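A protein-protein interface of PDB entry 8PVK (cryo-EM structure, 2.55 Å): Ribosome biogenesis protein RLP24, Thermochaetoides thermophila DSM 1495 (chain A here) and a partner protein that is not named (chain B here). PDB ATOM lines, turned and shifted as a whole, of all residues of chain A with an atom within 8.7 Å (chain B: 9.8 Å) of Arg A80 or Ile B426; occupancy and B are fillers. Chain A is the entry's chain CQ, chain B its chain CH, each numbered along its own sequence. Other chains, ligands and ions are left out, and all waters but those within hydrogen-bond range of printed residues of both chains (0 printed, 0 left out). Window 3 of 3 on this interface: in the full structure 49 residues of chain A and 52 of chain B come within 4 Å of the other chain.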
ATOM      1  N   VAL A  77     -13.882 -26.926 -11.467  1.00  0.00           N
ATOM      2  CA  VAL A  77     -14.385 -25.732 -10.799  1.00  0.00           C
ATOM      3  C   VAL A  77     -14.265 -25.961  -9.294  1.00  0.00           C
ATOM      4  O   VAL A  77     -15.023 -26.764  -8.730  1.00  0.00           O
ATOM      5  CB  VAL A  77     -15.831 -25.423 -11.205  1.00  0.00           C
ATOM      6  CG1 VAL A  77     -16.287 -24.116 -10.583  1.00  0.00           C
ATOM      7  CG2 VAL A  77     -15.951 -25.364 -12.718  1.00  0.00           C
ATOM      8  N   PRO A  78     -13.326 -25.306  -8.613  1.00  0.00           N
ATOM      9  CA  PRO A  78     -13.147 -25.546  -7.177  1.00  0.00           C
ATOM     10  C   PRO A  78     -14.303 -25.012  -6.347  1.00  0.00           C
ATOM     11  O   PRO A  78     -14.999 -24.069  -6.731  1.00  0.00           O
ATOM     12  CB  PRO A  78     -11.848 -24.802  -6.854  1.00  0.00           C
ATOM     13  CG  PRO A  78     -11.744 -23.757  -7.910  1.00  0.00           C
ATOM     14  CD  PRO A  78     -12.319 -24.375  -9.146  1.00  0.00           C
ATOM     15  N   VAL A  79     -14.493 -25.636  -5.190  1.00  0.00           N
ATOM     16  CA  VAL A  79     -15.523 -25.260  -4.231  1.00  0.00           C
ATOM     17  C   VAL A  79     -14.832 -24.770  -2.967  1.00  0.00           C
ATOM     18  O   VAL A  79     -13.824 -25.348  -2.542  1.00  0.00           O
ATOM     19  CB  VAL A  79     -16.467 -26.443  -3.928  1.00  0.00           C
ATOM     20  CG1 VAL A  79     -17.619 -26.013  -3.032  1.00  0.00           C
ATOM     21  CG2 VAL A  79     -16.993 -27.046  -5.219  1.00  0.00           C
ATOM     22  N   ARG A  80     -15.351 -23.684  -2.393  1.00  0.00           N
ATOM     23  CA  ARG A  80     -14.830 -23.166  -1.134  1.00  0.00           C
ATOM     24  C   ARG A  80     -14.988 -24.205  -0.030  1.00  0.00           C
ATOM     25  O   ARG A  80     -15.988 -24.926   0.026  1.00  0.00           O
ATOM     26  CB  ARG A  80     -15.558 -21.873  -0.760  1.00  0.00           C
ATOM     27  CG  ARG A  80     -14.943 -21.110   0.398  1.00  0.00           C
ATOM     28  CD  ARG A  80     -15.548 -19.722   0.521  1.00  0.00           C
ATOM     29  NE  ARG A  80     -15.355 -18.931  -0.687  1.00  0.00           N
ATOM     30  CZ  ARG A  80     -14.281 -18.194  -0.937  1.00  0.00           C
ATOM     31  NH1 ARG A  80     -13.276 -18.126  -0.080  1.00  0.00           N
ATOM     32  NH2 ARG A  80     -14.214 -17.509  -2.074  1.00  0.00           N
ATOM     33  N   TYR A  81     -13.983 -24.290   0.842  1.00  0.00           N
ATOM     34  CA  TYR A  81     -13.916 -25.375   1.812  1.00  0.00           C
ATOM     35  C   TYR A  81     -15.002 -25.230   2.872  1.00  0.00           C
ATOM     36  O   TYR A  81     -15.231 -24.139   3.403  1.00  0.00           O
ATOM     37  CB  TYR A  81     -12.538 -25.421   2.470  1.00  0.00           C
ATOM     38  CG  TYR A  81     -12.491 -26.296   3.701  1.00  0.00           C
ATOM     39  CD1 TYR A  81     -12.570 -27.677   3.591  1.00  0.00           C
ATOM     40  CD2 TYR A  81     -12.364 -25.745   4.970  1.00  0.00           C
ATOM     41  CE1 TYR A  81     -12.532 -28.486   4.706  1.00  0.00           C
ATOM     42  CE2 TYR A  81     -12.323 -26.547   6.092  1.00  0.00           C
ATOM     43  CZ  TYR A  81     -12.407 -27.916   5.954  1.00  0.00           C
ATOM     44  OH  TYR A  81     -12.367 -28.720   7.068  1.00  0.00           O
ATOM     45  N   ASN A  82     -15.667 -26.343   3.179  1.00  0.00           N
ATOM     46  CA  ASN A  82     -16.744 -26.376   4.162  1.00  0.00           C
ATOM     47  C   ASN A  82     -16.666 -27.706   4.898  1.00  0.00           C
ATOM     48  O   ASN A  82     -16.781 -28.768   4.274  1.00  0.00           O
ATOM     49  CB  ASN A  82     -18.108 -26.193   3.486  1.00  0.00           C
ATOM     50  CG  ASN A  82     -19.205 -25.809   4.461  1.00  0.00           C
ATOM     51  OD1 ASN A  82     -19.382 -26.437   5.503  1.00  0.00           O
ATOM     52  ND2 ASN A  82     -19.947 -24.761   4.124  1.00  0.00           N
ATOM     53  N   ARG A  83     -16.476 -27.637   6.221  1.00  0.00           N
ATOM     54  CA  ARG A  83     -16.207 -28.833   7.016  1.00  0.00           C
ATOM     55  C   ARG A  83     -17.362 -29.826   6.959  1.00  0.00           C
ATOM     56  O   ARG A  83     -17.143 -31.032   6.776  1.00  0.00           O
ATOM     57  CB  ARG A  83     -15.913 -28.439   8.464  1.00  0.00           C
ATOM     58  CG  ARG A  83     -15.432 -29.587   9.331  1.00  0.00           C
ATOM     59  CD  ARG A  83     -15.295 -29.173  10.786  1.00  0.00           C
ATOM     60  NE  ARG A  83     -14.261 -28.165  10.988  1.00  0.00           N
ATOM     61  CZ  ARG A  83     -13.903 -27.690  12.173  1.00  0.00           C
ATOM     62  NH1 ARG A  83     -14.482 -28.105  13.287  1.00  0.00           N
ATOM     63  NH2 ARG A  83     -12.939 -26.778  12.242  1.00  0.00           N
ATOM     64  N   LEU A  85     -19.553 -30.063   4.572  1.00  0.00           N
ATOM     65  CA  LEU A  85     -19.605 -30.592   3.214  1.00  0.00           C
ATOM     66  C   LEU A  85     -18.622 -31.740   3.031  1.00  0.00           C
ATOM     67  O   LEU A  85     -18.973 -32.777   2.461  1.00  0.00           O
ATOM     68  CB  LEU A  85     -19.326 -29.478   2.206  1.00  0.00           C
ATOM     69  CG  LEU A  85     -19.257 -29.892   0.735  1.00  0.00           C
ATOM     70  CD1 LEU A  85     -20.603 -30.418   0.268  1.00  0.00           C
ATOM     71  CD2 LEU A  85     -18.810 -28.726  -0.127  1.00  0.00           C
ATOM     72  N   TRP A  86     -17.394 -31.587   3.539  1.00  0.00           N
ATOM     73  CA  TRP A  86     -16.417 -32.676   3.463  1.00  0.00           C
ATOM     74  C   TRP A  86     -16.830 -33.899   4.285  1.00  0.00           C
ATOM     75  O   TRP A  86     -16.648 -35.037   3.830  1.00  0.00           O
ATOM     76  CB  TRP A  86     -15.031 -32.165   3.866  1.00  0.00           C
ATOM     77  CG  TRP A  86     -14.158 -31.771   2.690  1.00  0.00           C
ATOM     78  CD1 TRP A  86     -13.109 -32.486   2.190  1.00  0.00           C
ATOM     79  CD2 TRP A  86     -14.312 -30.638   1.820  1.00  0.00           C
ATOM     80  NE1 TRP A  86     -12.568 -31.848   1.104  1.00  0.00           N
ATOM     81  CE2 TRP A  86     -13.291 -30.714   0.852  1.00  0.00           C
ATOM     82  CE3 TRP A  86     -15.199 -29.563   1.776  1.00  0.00           C
ATOM     83  CZ2 TRP A  86     -13.136 -29.755  -0.146  1.00  0.00           C
ATOM     84  CZ3 TRP A  86     -15.043 -28.612   0.787  1.00  0.00           C
ATOM     85  CH2 TRP A  86     -14.019 -28.713  -0.160  1.00  0.00           C
ATOM     86  N   LEU B 421       0.064 -19.764   5.068  1.00  0.00           N
ATOM     87  CA  LEU B 421      -0.689 -19.600   3.831  1.00  0.00           C
ATOM     88  C   LEU B 421      -2.194 -19.573   4.051  1.00  0.00           C
ATOM     89  O   LEU B 421      -2.927 -19.115   3.168  1.00  0.00           O
ATOM     90  CB  LEU B 421      -0.336 -20.720   2.849  1.00  0.00           C
ATOM     91  CG  LEU B 421       1.093 -20.721   2.307  1.00  0.00           C
ATOM     92  CD1 LEU B 421       1.318 -21.920   1.400  1.00  0.00           C
ATOM     93  CD2 LEU B 421       1.389 -19.425   1.573  1.00  0.00           C
ATOM     94  N   ARG B 422      -2.670 -20.043   5.200  1.00  0.00           N
ATOM     95  CA  ARG B 422      -4.093 -20.079   5.501  1.00  0.00           C
ATOM     96  C   ARG B 422      -4.570 -18.845   6.254  1.00  0.00           C
ATOM     97  O   ARG B 422      -5.734 -18.798   6.661  1.00  0.00           O
ATOM     98  CB  ARG B 422      -4.428 -21.338   6.304  1.00  0.00           C
ATOM     99  CG  ARG B 422      -4.436 -22.612   5.480  1.00  0.00           C
ATOM    100  CD  ARG B 422      -4.184 -23.826   6.350  1.00  0.00           C
ATOM    101  NE  ARG B 422      -4.184 -25.063   5.580  1.00  0.00           N
ATOM    102  CZ  ARG B 422      -5.125 -25.994   5.662  1.00  0.00           C
ATOM    103  NH1 ARG B 422      -6.163 -25.858   6.469  1.00  0.00           N
ATOM    104  NH2 ARG B 422      -5.017 -27.091   4.917  1.00  0.00           N
ATOM    105  N   LYS B 423      -3.697 -17.854   6.452  1.00  0.00           N
ATOM    106  CA  LYS B 423      -4.074 -16.661   7.205  1.00  0.00           C
ATOM    107  C   LYS B 423      -5.087 -15.814   6.443  1.00  0.00           C
ATOM    108  O   LYS B 423      -6.003 -15.243   7.045  1.00  0.00           O
ATOM    109  CB  LYS B 423      -2.826 -15.843   7.536  1.00  0.00           C
ATOM    110  CG  LYS B 423      -3.083 -14.618   8.395  1.00  0.00           C
ATOM    111  CD  LYS B 423      -1.787 -13.895   8.719  1.00  0.00           C
ATOM    112  CE  LYS B 423      -2.028 -12.722   9.656  1.00  0.00           C
ATOM    113  NZ  LYS B 423      -2.810 -11.638   8.998  1.00  0.00           N
ATOM    114  N   ASP B 424      -4.945 -15.728   5.120  1.00  0.00           N
ATOM    115  CA  ASP B 424      -5.821 -14.912   4.290  1.00  0.00           C
ATOM    116  C   ASP B 424      -6.954 -15.717   3.664  1.00  0.00           C
ATOM    117  O   ASP B 424      -7.550 -15.271   2.679  1.00  0.00           O
ATOM    118  CB  ASP B 424      -5.011 -14.207   3.203  1.00  0.00           C
ATOM    119  CG  ASP B 424      -4.207 -13.040   3.739  1.00  0.00           C
ATOM    120  OD1 ASP B 424      -4.385 -12.691   4.924  1.00  0.00           O
ATOM    121  OD2 ASP B 424      -3.399 -12.471   2.975  1.00  0.00           O
ATOM    122  N   TRP B 425      -7.257 -16.892   4.210  1.00  0.00           N
ATOM    123  CA  TRP B 425      -8.367 -17.688   3.704  1.00  0.00           C
ATOM    124  C   TRP B 425      -9.695 -17.056   4.100  1.00  0.00           C
ATOM    125  O   TRP B 425      -9.895 -16.679   5.258  1.00  0.00           O
ATOM    126  CB  TRP B 425      -8.284 -19.116   4.240  1.00  0.00           C
ATOM    127  CG  TRP B 425      -7.516 -20.052   3.361  1.00  0.00           C
ATOM    128  CD1 TRP B 425      -6.693 -19.717   2.328  1.00  0.00           C
ATOM    129  CD2 TRP B 425      -7.500 -21.482   3.440  1.00  0.00           C
ATOM    130  NE1 TRP B 425      -6.167 -20.849   1.757  1.00  0.00           N
ATOM    131  CE2 TRP B 425      -6.646 -21.946   2.422  1.00  0.00           C
ATOM    132  CE3 TRP B 425      -8.128 -22.414   4.272  1.00  0.00           C
ATOM    133  CZ2 TRP B 425      -6.401 -23.301   2.214  1.00  0.00           C
ATOM    134  CZ3 TRP B 425      -7.883 -23.758   4.065  1.00  0.00           C
ATOM    135  CH2 TRP B 425      -7.027 -24.190   3.044  1.00  0.00           C
ATOM    136  N   ILE B 426     -10.601 -16.943   3.136  1.00  0.00           N
ATOM    137  CA  ILE B 426     -11.941 -16.418   3.367  1.00  0.00           C
ATOM    138  C   ILE B 426     -12.895 -17.603   3.406  1.00  0.00           C
ATOM    139  O   ILE B 426     -13.230 -18.179   2.364  1.00  0.00           O
ATOM    140  CB  ILE B 426     -12.350 -15.411   2.286  1.00  0.00           C
ATOM    141  CG1 ILE B 426     -11.288 -14.320   2.140  1.00  0.00           C
ATOM    142  CG2 ILE B 426     -13.703 -14.801   2.612  1.00  0.00           C
ATOM    143  CD1 ILE B 426     -11.421 -13.512   0.869  1.00  0.00           C
ATOM    144  N   LEU B 427     -13.335 -17.973   4.603  1.00  0.00           N
ATOM    145  CA  LEU B 427     -14.242 -19.092   4.794  1.00  0.00           C
ATOM    146  C   LEU B 427     -15.514 -18.619   5.483  1.00  0.00           C
ATOM    147  O   LEU B 427     -15.574 -17.518   6.035  1.00  0.00           O
ATOM    148  CB  LEU B 427     -13.587 -20.210   5.616  1.00  0.00           C
ATOM    149  CG  LEU B 427     -12.319 -20.838   5.035  1.00  0.00           C
ATOM    150  CD1 LEU B 427     -11.850 -21.987   5.907  1.00  0.00           C
ATOM    151  CD2 LEU B 427     -12.555 -21.311   3.610  1.00  0.00           C
ATOM    152  N   GLU B 428     -16.542 -19.470   5.426  1.00  0.00           N
ATOM    153  CA  GLU B 428     -17.802 -19.165   6.096  1.00  0.00           C
ATOM    154  C   GLU B 428     -17.632 -19.129   7.610  1.00  0.00           C
ATOM    155  O   GLU B 428     -18.210 -18.269   8.284  1.00  0.00           O
ATOM    156  CB  GLU B 428     -18.876 -20.184   5.701  1.00  0.00           C
ATOM    157  CG  GLU B 428     -19.192 -20.281   4.201  1.00  0.00           C
ATOM    158  CD  GLU B 428     -18.233 -21.169   3.412  1.00  0.00           C
ATOM    159  OE1 GLU B 428     -17.072 -21.352   3.835  1.00  0.00           O
ATOM    160  OE2 GLU B 428     -18.651 -21.690   2.356  1.00  0.00           O
ATOM    161  N   ASN B 429     -16.847 -20.051   8.161  1.00  0.00           N
ATOM    162  CA  ASN B 429     -16.611 -20.118   9.598  1.00  0.00           C
ATOM    163  C   ASN B 429     -15.118 -19.983   9.866  1.00  0.00           C
ATOM    164  O   ASN B 429     -14.339 -20.861   9.455  1.00  0.00           O
ATOM    165  CB  ASN B 429     -17.147 -21.429  10.172  1.00  0.00           C
ATOM    166  CG  ASN B 429     -17.346 -21.370  11.668  1.00  0.00           C
ATOM    167  OD1 ASN B 429     -17.327 -20.295  12.267  1.00  0.00           O
ATOM    168  ND2 ASN B 429     -17.541 -22.530  12.283  1.00  0.00           N
ATOM    169  N   PRO B 430     -14.676 -18.924  10.556  1.00  0.00           N
ATOM    170  CA  PRO B 430     -13.233 -18.650  10.671  1.00  0.00           C
ATOM    171  C   PRO B 430     -12.442 -19.675  11.474  1.00  0.00           C
ATOM    172  O   PRO B 430     -11.206 -19.614  11.453  1.00  0.00           O
ATOM    173  CB  PRO B 430     -13.192 -17.277  11.355  1.00  0.00           C
ATOM    174  CG  PRO B 430     -14.519 -16.665  11.055  1.00  0.00           C
ATOM    175  CD  PRO B 430     -15.487 -17.806  11.066  1.00  0.00           C
ATOM    176  N   GLU B 431     -13.088 -20.601  12.178  1.00  0.00           N
ATOM    177  CA  GLU B 431     -12.363 -21.666  12.855  1.00  0.00           C
ATOM    178  C   GLU B 431     -12.175 -22.899  11.980  1.00  0.00           C
ATOM    179  O   GLU B 431     -11.666 -23.914  12.463  1.00  0.00           O
ATOM    180  CB  GLU B 431     -13.058 -22.049  14.166  1.00  0.00           C
ATOM    181  CG  GLU B 431     -14.502 -22.486  14.033  1.00  0.00           C
ATOM    182  CD  GLU B 431     -15.467 -21.417  14.496  1.00  0.00           C
ATOM    183  OE1 GLU B 431     -15.047 -20.248  14.617  1.00  0.00           O
ATOM    184  OE2 GLU B 431     -16.645 -21.746  14.747  1.00  0.00           O
ATOM    185  N   TRP B 432     -12.573 -22.836  10.710  1.00  0.00           N
ATOM    186  CA  TRP B 432     -12.241 -23.880   9.749  1.00  0.00           C
ATOM    187  C   TRP B 432     -10.943 -23.601   9.006  1.00  0.00           C
ATOM    188  O   TRP B 432     -10.554 -24.399   8.147  1.00  0.00           O
ATOM    189  CB  TRP B 432     -13.366 -24.055   8.725  1.00  0.00           C
ATOM    190  CG  TRP B 432     -14.692 -24.435   9.291  1.00  0.00           C
ATOM    191  CD1 TRP B 432     -14.943 -24.947  10.529  1.00  0.00           C
ATOM    192  CD2 TRP B 432     -15.956 -24.346   8.629  1.00  0.00           C
ATOM    193  NE1 TRP B 432     -16.289 -25.177  10.681  1.00  0.00           N
ATOM    194  CE2 TRP B 432     -16.932 -24.818   9.525  1.00  0.00           C
ATOM    195  CE3 TRP B 432     -16.358 -23.909   7.363  1.00  0.00           C
ATOM    196  CZ2 TRP B 432     -18.284 -24.860   9.201  1.00  0.00           C
ATOM    197  CZ3 TRP B 432     -17.699 -23.957   7.040  1.00  0.00           C
ATOM    198  CH2 TRP B 432     -18.646 -24.427   7.956  1.00  0.00           C
ATOM    199  N   LYS B 433     -10.267 -22.491   9.311  1.00  0.00           N
ATOM    200  CA  LYS B 433      -9.125 -22.055   8.516  1.00  0.00           C
ATOM    201  C   LYS B 433      -7.895 -22.931   8.710  1.00  0.00           C
ATOM    202  O   LYS B 433      -7.029 -22.958   7.831  1.00  0.00           O
ATOM    203  CB  LYS B 433      -8.787 -20.602   8.849  1.00  0.00           C
ATOM    204  CG  LYS B 433      -9.721 -19.592   8.196  1.00  0.00           C
ATOM    205  CD  LYS B 433      -9.449 -18.155   8.638  1.00  0.00           C
ATOM    206  CE  LYS B 433      -7.972 -17.875   8.863  1.00  0.00           C
ATOM    207  NZ  LYS B 433      -7.700 -16.416   8.955  1.00  0.00           N
ATOM    208  N   ILE B 437      -7.665 -30.956   5.781  1.00  0.00           N
ATOM    209  CA  ILE B 437      -8.667 -31.298   4.774  1.00  0.00           C
ATOM    210  C   ILE B 437      -8.398 -32.707   4.260  1.00  0.00           C
ATOM    211  O   ILE B 437      -7.289 -32.990   3.786  1.00  0.00           O
ATOM    212  CB  ILE B 437      -8.665 -30.277   3.627  1.00  0.00           C
ATOM    213  CG1 ILE B 437      -8.906 -28.870   4.173  1.00  0.00           C
ATOM    214  CG2 ILE B 437      -9.722 -30.630   2.600  1.00  0.00           C
ATOM    215  CD1 ILE B 437      -8.734 -27.778   3.144  1.00  0.00           C
ATOM    216  N   TYR B 447     -11.732 -35.160  -3.276  1.00  0.00           N
ATOM    217  CA  TYR B 447     -11.968 -34.047  -4.188  1.00  0.00           C
ATOM    218  C   TYR B 447     -12.678 -34.481  -5.464  1.00  0.00           C
ATOM    219  O   TYR B 447     -13.315 -33.648  -6.115  1.00  0.00           O
ATOM    220  CB  TYR B 447     -10.644 -33.363  -4.532  1.00  0.00           C
ATOM    221  CG  TYR B 447     -10.165 -32.403  -3.469  1.00  0.00           C
ATOM    222  CD1 TYR B 447      -9.549 -32.869  -2.314  1.00  0.00           C
ATOM    223  CD2 TYR B 447     -10.330 -31.032  -3.617  1.00  0.00           C
ATOM    224  CE1 TYR B 447      -9.110 -31.997  -1.337  1.00  0.00           C
ATOM    225  CE2 TYR B 447      -9.892 -30.151  -2.646  1.00  0.00           C
ATOM    226  CZ  TYR B 447      -9.283 -30.640  -1.508  1.00  0.00           C
ATOM    227  OH  TYR B 447      -8.846 -29.769  -0.538  1.00  0.00           O
ATOM    228  N   ILE B 450     -16.316 -34.334  -4.149  1.00  0.00           N
ATOM    229  CA  ILE B 450     -16.831 -33.065  -3.639  1.00  0.00           C
ATOM    230  C   ILE B 450     -17.754 -32.444  -4.680  1.00  0.00           C
ATOM    231  O   ILE B 450     -17.347 -32.174  -5.816  1.00  0.00           O
ATOM    232  CB  ILE B 450     -15.689 -32.113  -3.266  1.00  0.00           C
ATOM    233  CG1 ILE B 450     -15.013 -32.577  -1.978  1.00  0.00           C
ATOM    234  CG2 ILE B 450     -16.204 -30.689  -3.097  1.00  0.00           C
ATOM    235  CD1 ILE B 450     -15.893 -32.443  -0.757  1.00  0.00           C
ATOM    236  N   ASP B 451     -19.011 -32.216  -4.292  1.00  0.00           N
ATOM    237  CA  ASP B 451     -20.038 -31.667  -5.153  1.00  0.00           C
ATOM    238  C   ASP B 451     -20.948 -30.841  -4.252  1.00  0.00           C
ATOM    239  O   ASP B 451     -21.386 -31.355  -3.212  1.00  0.00           O
ATOM    240  CB  ASP B 451     -20.838 -32.762  -5.862  1.00  0.00           C
ATOM    241  CG  ASP B 451     -21.776 -32.215  -6.920  1.00  0.00           C
ATOM    242  OD1 ASP B 451     -21.372 -31.297  -7.663  1.00  0.00           O
ATOM    243  OD2 ASP B 451     -22.918 -32.710  -7.012  1.00  0.00           O
ATOM    244  N   PRO B 452     -21.208 -29.571  -4.591  1.00  0.00           N
ATOM    245  CA  PRO B 452     -22.070 -28.745  -3.722  1.00  0.00           C
ATOM    246  C   PRO B 452     -23.490 -29.270  -3.574  1.00  0.00           C
ATOM    247  O   PRO B 452     -24.061 -29.193  -2.479  1.00  0.00           O
ATOM    248  CB  PRO B 452     -22.041 -27.370  -4.407  1.00  0.00           C
ATOM    249  CG  PRO B 452     -21.547 -27.626  -5.794  1.00  0.00           C
ATOM    250  CD  PRO B 452     -20.628 -28.794  -5.696  1.00  0.00           C
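Of the 9 printed residues of chain A, 6 touch a printed residue of chain B.
Along chain A the printed residues that touch a printed residue of chain B span positions 80 to 86.
Among the printed residues, 13 pairs touch across the chains.
Among the printed residues, no Asp or Glu carboxylate lies within 4 Å of a Lys or Arg side-chain nitrogen of the other chain.
Among the printed residues, pairs that only touch across the chains: Arg A80 with Glu B428 (3.995 Å), Tyr A81 with Leu B427 (3.9 Å), Tyr A81 with Trp B432 (3.5 Å), Tyr A81 with Ile B437 (3.7 Å), Asn A82 with Glu B428 (3.8 Å), Asn A82 with Trp B432 (3.3 Å), Arg A83 with Trp B432 (3.2 Å), Leu A85 with Asp B451 (3.7 Å), Trp A86 with Ile B437 (3.4 Å) and Trp A86 with Ile B450 (3.5 Å).
The side-chain amide nitrogen of Asn B429 lies within hydrogen-bond range of the side-chain carboxylate of Glu B431 (2.7 Å).
NE1 of Trp B432 lies close to ND2 of Asn B429 (3.3 Å).
The backbone carbonyl oxygen of Ile B426 is in hydrogen-bond range of the guanidinium group of Arg A80 (2.4 Å).
The guanidinium group of Arg A83 sits at hydrogen-bond distance from the backbone carbonyl oxygen of Glu B431, at 3.1 Å.
O of Tyr A81 sits close to OE1 of Glu B428 (3.4 Å).
Of the printed residues of chain B, Arg A80 touches Ile B426 and Glu B428.
Ile B426 touches one residue of chain A.
No residue of chain B comes within 4 Å of Val A79.
Of the printed residues of chain A, Ile B437 touches Tyr A81 and Trp A86.
Printed residues of chain B within 4 Å of Arg A83: Glu B431 and Trp B432.
Of the printed residues of chain B, Asn A82 touches Glu B428 (3.8 Å) and Trp B432 (3.3 Å).
Of the printed residues of chain A, Asp B451 touches Leu A85.
Arg B422 touches none of the printed residues of chain A.
Leu B421 touches none of the printed residues of chain A.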
